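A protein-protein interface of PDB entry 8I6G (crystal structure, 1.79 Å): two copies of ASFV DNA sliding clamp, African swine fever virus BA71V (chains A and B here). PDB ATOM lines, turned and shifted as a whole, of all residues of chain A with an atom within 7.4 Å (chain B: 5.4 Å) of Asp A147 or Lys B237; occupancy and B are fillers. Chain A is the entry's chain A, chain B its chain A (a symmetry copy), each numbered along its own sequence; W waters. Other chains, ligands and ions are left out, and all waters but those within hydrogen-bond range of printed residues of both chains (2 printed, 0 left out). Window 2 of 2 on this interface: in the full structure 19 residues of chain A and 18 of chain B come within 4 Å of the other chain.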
ATOM      1  N   THR A 142     -20.968   0.552 -11.267  1.00  0.00           N
ATOM      2  CA  THR A 142     -20.541   1.385 -12.385  1.00  0.00           C
ATOM      3  C   THR A 142     -19.687   0.649 -13.415  1.00  0.00           C
ATOM      4  O   THR A 142     -18.683   0.022 -13.073  1.00  0.00           O
ATOM      5  CB  THR A 142     -19.749   2.591 -11.883  1.00  0.00           C
ATOM      6  OG1 THR A 142     -20.454   3.199 -10.799  1.00  0.00           O
ATOM      7  CG2 THR A 142     -19.572   3.601 -12.997  1.00  0.00           C
ATOM      8  N   ASP A 143     -20.113   0.722 -14.673  1.00  0.00           N
ATOM      9  CA  ASP A 143     -19.334   0.254 -15.815  1.00  0.00           C
ATOM     10  C   ASP A 143     -18.713   1.484 -16.466  1.00  0.00           C
ATOM     11  O   ASP A 143     -19.425   2.314 -17.030  1.00  0.00           O
ATOM     12  CB  ASP A 143     -20.225  -0.520 -16.801  1.00  0.00           C
ATOM     13  CG  ASP A 143     -19.476  -1.015 -18.040  1.00  0.00           C
ATOM     14  OD1 ASP A 143     -18.359  -0.542 -18.331  1.00  0.00           O
ATOM     15  OD2 ASP A 143     -20.031  -1.885 -18.750  1.00  0.00           O
ATOM     16  N   PHE A 144     -17.388   1.597 -16.388  1.00  0.00           N
ATOM     17  CA  PHE A 144     -16.701   2.815 -16.814  1.00  0.00           C
ATOM     18  C   PHE A 144     -16.377   2.839 -18.300  1.00  0.00           C
ATOM     19  O   PHE A 144     -16.054   3.889 -18.852  1.00  0.00           O
ATOM     20  CB  PHE A 144     -15.420   3.001 -16.010  1.00  0.00           C
ATOM     21  CG  PHE A 144     -15.662   3.379 -14.590  1.00  0.00           C
ATOM     22  CD1 PHE A 144     -15.901   4.700 -14.246  1.00  0.00           C
ATOM     23  CD2 PHE A 144     -15.667   2.418 -13.594  1.00  0.00           C
ATOM     24  CE1 PHE A 144     -16.129   5.059 -12.933  1.00  0.00           C
ATOM     25  CE2 PHE A 144     -15.895   2.771 -12.272  1.00  0.00           C
ATOM     26  CZ  PHE A 144     -16.127   4.093 -11.943  1.00  0.00           C
ATOM     27  N   ASP A 145     -16.466   1.680 -18.942  1.00  0.00           N
ATOM     28  CA  ASP A 145     -16.245   1.587 -20.377  1.00  0.00           C
ATOM     29  C   ASP A 145     -17.289   2.378 -21.151  1.00  0.00           C
ATOM     30  O   ASP A 145     -16.985   2.965 -22.185  1.00  0.00           O
ATOM     31  CB  ASP A 145     -16.267   0.133 -20.831  1.00  0.00           C
ATOM     32  CG  ASP A 145     -14.971  -0.589 -20.533  1.00  0.00           C
ATOM     33  OD1 ASP A 145     -14.104  -0.005 -19.843  1.00  0.00           O
ATOM     34  OD2 ASP A 145     -14.817  -1.741 -20.992  1.00  0.00           O
ATOM     35  N   ILE A 146     -18.520   2.385 -20.653  1.00  0.00           N
ATOM     36  CA  ILE A 146     -19.607   3.034 -21.374  1.00  0.00           C
ATOM     37  C   ILE A 146     -20.415   4.008 -20.521  1.00  0.00           C
ATOM     38  O   ILE A 146     -21.525   4.373 -20.896  1.00  0.00           O
ATOM     39  CB  ILE A 146     -20.579   2.001 -21.959  1.00  0.00           C
ATOM     40  CG1 ILE A 146     -20.984   0.990 -20.885  1.00  0.00           C
ATOM     41  CG2 ILE A 146     -19.952   1.300 -23.169  1.00  0.00           C
ATOM     42  CD1 ILE A 146     -22.164   0.134 -21.274  1.00  0.00           C
ATOM     43  N   ASP A 147     -19.858   4.427 -19.386  1.00  0.00           N
ATOM     44  CA  ASP A 147     -20.551   5.335 -18.464  1.00  0.00           C
ATOM     45  C   ASP A 147     -21.956   4.847 -18.115  1.00  0.00           C
ATOM     46  O   ASP A 147     -22.931   5.610 -18.180  1.00  0.00           O
ATOM     47  CB  ASP A 147     -20.627   6.749 -19.045  1.00  0.00           C
ATOM     48  CG  ASP A 147     -19.258   7.348 -19.289  1.00  0.00           C
ATOM     49  OD1 ASP A 147     -18.266   6.779 -18.784  1.00  0.00           O
ATOM     50  OD2 ASP A 147     -19.171   8.396 -19.969  1.00  0.00           O
ATOM     51  N   LYS A 148     -22.042   3.569 -17.762  1.00  0.00           N
ATOM     52  CA  LYS A 148     -23.290   2.943 -17.361  1.00  0.00           C
ATOM     53  C   LYS A 148     -23.335   2.815 -15.853  1.00  0.00           C
ATOM     54  O   LYS A 148     -22.382   2.323 -15.241  1.00  0.00           O
ATOM     55  CB  LYS A 148     -23.442   1.557 -18.003  1.00  0.00           C
ATOM     56  CG  LYS A 148     -24.592   0.742 -17.419  1.00  0.00           C
ATOM     57  CD  LYS A 148     -24.816  -0.562 -18.184  1.00  0.00           C
ATOM     58  CE  LYS A 148     -24.097  -1.726 -17.575  1.00  0.00           C
ATOM     59  NZ  LYS A 148     -24.589  -3.043 -18.108  1.00  0.00           N
ATOM     60  N   GLU A 149     -24.449   3.228 -15.265  1.00  0.00           N
ATOM     61  CA  GLU A 149     -24.621   3.184 -13.831  1.00  0.00           C
ATOM     62  C   GLU A 149     -25.868   2.383 -13.483  1.00  0.00           C
ATOM     63  O   GLU A 149     -26.967   2.680 -13.953  1.00  0.00           O
ATOM     64  CB  GLU A 149     -24.703   4.611 -13.298  1.00  0.00           C
ATOM     65  CG  GLU A 149     -24.561   4.772 -11.838  1.00  0.00           C
ATOM     66  CD  GLU A 149     -24.573   6.244 -11.474  1.00  0.00           C
ATOM     67  OE1 GLU A 149     -25.674   6.787 -11.240  1.00  0.00           O
ATOM     68  OE2 GLU A 149     -23.487   6.863 -11.466  1.00  0.00           O
ATOM     69  N   MET B 231     -28.706   3.516 -16.034  1.00  0.00           N
ATOM     70  CA  MET B 231     -28.612   4.812 -16.702  1.00  0.00           C
ATOM     71  C   MET B 231     -27.352   4.918 -17.551  1.00  0.00           C
ATOM     72  O   MET B 231     -26.242   4.644 -17.090  1.00  0.00           O
ATOM     73  CB  MET B 231     -28.649   5.942 -15.677  1.00  0.00           C
ATOM     74  CG  MET B 231     -28.737   7.308 -16.331  1.00  0.00           C
ATOM     75  SD  MET B 231     -28.481   8.590 -15.110  1.00  0.00           S
ATOM     76  CE  MET B 231     -29.933   8.420 -14.155  1.00  0.00           C
ATOM     77  N   TYR B 232     -27.541   5.304 -18.802  1.00  0.00           N
ATOM     78  CA  TYR B 232     -26.462   5.487 -19.756  1.00  0.00           C
ATOM     79  C   TYR B 232     -26.174   6.973 -19.945  1.00  0.00           C
ATOM     80  O   TYR B 232     -26.895   7.665 -20.666  1.00  0.00           O
ATOM     81  CB  TYR B 232     -26.828   4.827 -21.090  1.00  0.00           C
ATOM     82  CG  TYR B 232     -26.889   3.323 -20.937  1.00  0.00           C
ATOM     83  CD1 TYR B 232     -28.044   2.695 -20.479  1.00  0.00           C
ATOM     84  CD2 TYR B 232     -25.776   2.544 -21.191  1.00  0.00           C
ATOM     85  CE1 TYR B 232     -28.086   1.316 -20.305  1.00  0.00           C
ATOM     86  CE2 TYR B 232     -25.810   1.165 -21.021  1.00  0.00           C
ATOM     87  CZ  TYR B 232     -26.971   0.567 -20.586  1.00  0.00           C
ATOM     88  OH  TYR B 232     -27.010  -0.794 -20.404  1.00  0.00           O
ATOM     89  N   LYS B 233     -25.107   7.427 -19.296  1.00  0.00           N
ATOM     90  CA  LYS B 233     -24.773   8.841 -19.180  1.00  0.00           C
ATOM     91  C   LYS B 233     -24.121   9.440 -20.419  1.00  0.00           C
ATOM     92  O   LYS B 233     -24.198  10.652 -20.629  1.00  0.00           O
ATOM     93  CB  LYS B 233     -23.851   9.044 -17.983  1.00  0.00           C
ATOM     94  CG  LYS B 233     -24.538   8.857 -16.662  1.00  0.00           C
ATOM     95  CD  LYS B 233     -23.593   9.218 -15.515  1.00  0.00           C
ATOM     96  CE  LYS B 233     -24.264   9.055 -14.170  1.00  0.00           C
ATOM     97  NZ  LYS B 233     -23.320   8.458 -13.175  1.00  0.00           N
ATOM     98  N   SER B 234     -23.476   8.601 -21.222  1.00  0.00           N
ATOM     99  CA  SER B 234     -22.818   9.052 -22.439  1.00  0.00           C
ATOM    100  C   SER B 234     -23.460   8.435 -23.676  1.00  0.00           C
ATOM    101  O   SER B 234     -23.193   7.277 -24.003  1.00  0.00           O
ATOM    102  CB  SER B 234     -21.328   8.712 -22.389  1.00  0.00           C
ATOM    103  OG  SER B 234     -20.795   8.570 -23.697  1.00  0.00           O
ATOM    104  N   SER B 235     -24.307   9.200 -24.360  1.00  0.00           N
ATOM    105  CA  SER B 235     -24.951   8.703 -25.572  1.00  0.00           C
ATOM    106  C   SER B 235     -23.933   8.240 -26.613  1.00  0.00           C
ATOM    107  O   SER B 235     -24.163   7.256 -27.317  1.00  0.00           O
ATOM    108  CB  SER B 235     -25.867   9.778 -26.172  1.00  0.00           C
ATOM    109  OG  SER B 235     -26.886  10.145 -25.256  1.00  0.00           O
ATOM    110  N   ASN B 236     -22.805   8.940 -26.694  1.00  0.00           N
ATOM    111  CA  ASN B 236     -21.771   8.636 -27.683  1.00  0.00           C
ATOM    112  C   ASN B 236     -21.211   7.231 -27.558  1.00  0.00           C
ATOM    113  O   ASN B 236     -20.901   6.577 -28.551  1.00  0.00           O
ATOM    114  CB  ASN B 236     -20.622   9.644 -27.568  1.00  0.00           C
ATOM    115  N   LYS B 237     -21.078   6.770 -26.321  1.00  0.00           N
ATOM    116  CA  LYS B 237     -20.412   5.503 -26.064  1.00  0.00           C
ATOM    117  C   LYS B 237     -21.271   4.292 -26.413  1.00  0.00           C
ATOM    118  O   LYS B 237     -20.752   3.184 -26.557  1.00  0.00           O
ATOM    119  CB  LYS B 237     -19.967   5.447 -24.601  1.00  0.00           C
ATOM    120  CG  LYS B 237     -18.692   6.227 -24.366  1.00  0.00           C
ATOM    121  CD  LYS B 237     -18.376   6.371 -22.900  1.00  0.00           C
ATOM    122  CE  LYS B 237     -17.022   7.029 -22.715  1.00  0.00           C
ATOM    123  NZ  LYS B 237     -16.795   7.414 -21.301  1.00  0.00           N
ATOM    124  N   ILE B 238     -22.578   4.490 -26.552  1.00  0.00           N
ATOM    125  CA  ILE B 238     -23.448   3.406 -27.003  1.00  0.00           C
ATOM    126  C   ILE B 238     -24.063   3.760 -28.365  1.00  0.00           C
ATOM    127  O   ILE B 238     -25.072   3.183 -28.776  1.00  0.00           O
ATOM    128  CB  ILE B 238     -24.566   3.080 -25.959  1.00  0.00           C
ATOM    129  CG1 ILE B 238     -25.400   4.320 -25.618  1.00  0.00           C
ATOM    130  CG2 ILE B 238     -23.957   2.465 -24.692  1.00  0.00           C
ATOM    131  CD1 ILE B 238     -26.682   3.985 -24.854  1.00  0.00           C
ATOM    132  N   ASN B 239     -23.443   4.706 -29.067  1.00  0.00           N
ATOM    133  CA  ASN B 239     -23.923   5.116 -30.388  1.00  0.00           C
ATOM    134  C   ASN B 239     -25.413   5.429 -30.432  1.00  0.00           C
ATOM    135  O   ASN B 239     -26.114   5.004 -31.351  1.00  0.00           O
ATOM    136  CB  ASN B 239     -23.616   4.023 -31.417  1.00  0.00           C
ATOM    137  CG  ASN B 239     -22.192   4.072 -31.911  1.00  0.00           C
ATOM    138  OD1 ASN B 239     -21.306   3.425 -31.355  1.00  0.00           O
ATOM    139  ND2 ASN B 239     -21.961   4.842 -32.975  1.00  0.00           N
HETATM  140  O   HOH W   1     -23.526   5.707 -21.566  1.00  0.00           O
HETATM  141  O   HOH W   2     -25.128  -3.014 -21.037  1.00  0.00           O
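The backbone carbonyl oxygen (O) of Asp A147 lies within hydrogen-bond range of the backbone NH (N) of Lys B233 (3.0 Å).
The side-chain amino group (NZ) of Lys B237 is in salt-bridge range of the side-chain carboxylate (OD2) of Asp A147, at 2.9 Å.
The backbone NH (N) of Met B231 sits at hydrogen-bond distance from the backbone carbonyl oxygen (O) of Glu A149.
OE1 of Glu A149 is in salt-bridge range of NZ of Lys B233, at 3.5 Å.
Asp A147 touches five residues of chain B.
Of the printed residues of chain A, Lys B237 touches Asp A145 (3.7 Å), Ile A146 (3.9 Å) and Asp A147 (2.9 Å).
Of the printed residues of chain B, Lys A148 touches Met B231 and Tyr B232.
Of the printed residues of chain B, Ile A146 touches Tyr B232 and Lys B237.
Printed residues of chain A within 4 Å of Tyr B232: Ile A146 (3.8 Å), Asp A147 (3.9 Å) and Lys A148 (3.1 Å).
Ser B235 touches none of the printed residues of chain A.
The nearest printed residue of chain A that does not touch Lys B233 is Ile A146 (5.0 Å).
No position is printed for both chains.
Of the 12 pairs that touch across the chains among the printed residues, none has its exchanged pair printed and touching as well.
Asp A145 touches Lys B237 (O to CD, 3.7 Å).
CD1 of Ile A146 touches CE2 of Tyr B232, 3.8 Å away.
CD of Lys B237 touches CA of Ile A146, at 3.9 Å.
O of Asp A147 touches O of Met B231, at 3.6 Å.
Asp A147 touches Tyr B232 (O to CA, 3.9 Å).
Asp A147 touches Ser B234.
Lys A148 touches Met B231.
OH of Tyr B232 touches CD of Lys A148, 3.1 Å away.
Of the 9 printed residues of chain B, 5 touch a printed residue of chain A.
Hydrophobic or aromatic side chains of chain B that line the printed part of chain A: Tyr B232.
Printed residues of chain A that touch a printed residue of chain B: Asp A145, Ile A146, Asp A147, Lys A148 and Glu A149.
Hydrophobic or aromatic side chains of chain A within 4 Å of the printed part of chain B: Ile A146.
Along chain A the printed residues that touch a printed residue of chain B span positions 145 to 149.
Among the printed residues, Asp or Glu carboxylates within 4 Å of a Lys or Arg side-chain nitrogen of the other chain: Asp A147 with Lys B237 (2.9 Å) and Glu A149 with Lys B233 (2.3 Å).
Water W1 lies within hydrogen-bond range of O of Ile A146 (2.5 Å), N of Ser B234 (2.9 Å), N of Lys B233 (3.3 Å) and O of Asp A147 (3.4 Å).
Water W2 bridges OH of Tyr B232 (3.0 Å) and NZ of Lys A148 (3.0 Å).
The backbone NH (N) of Asp A145 is in hydrogen-bond range of the side-chain carboxylate (OD1) of Asp A143.
The backbone NH (N) of Asp A143 lies within hydrogen-bond range of the backbone carbonyl oxygen (O) of Lys A148 (2.8 Å).
N of Lys B237 is in hydrogen-bond range of OG of Ser B234 (3.2 Å).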
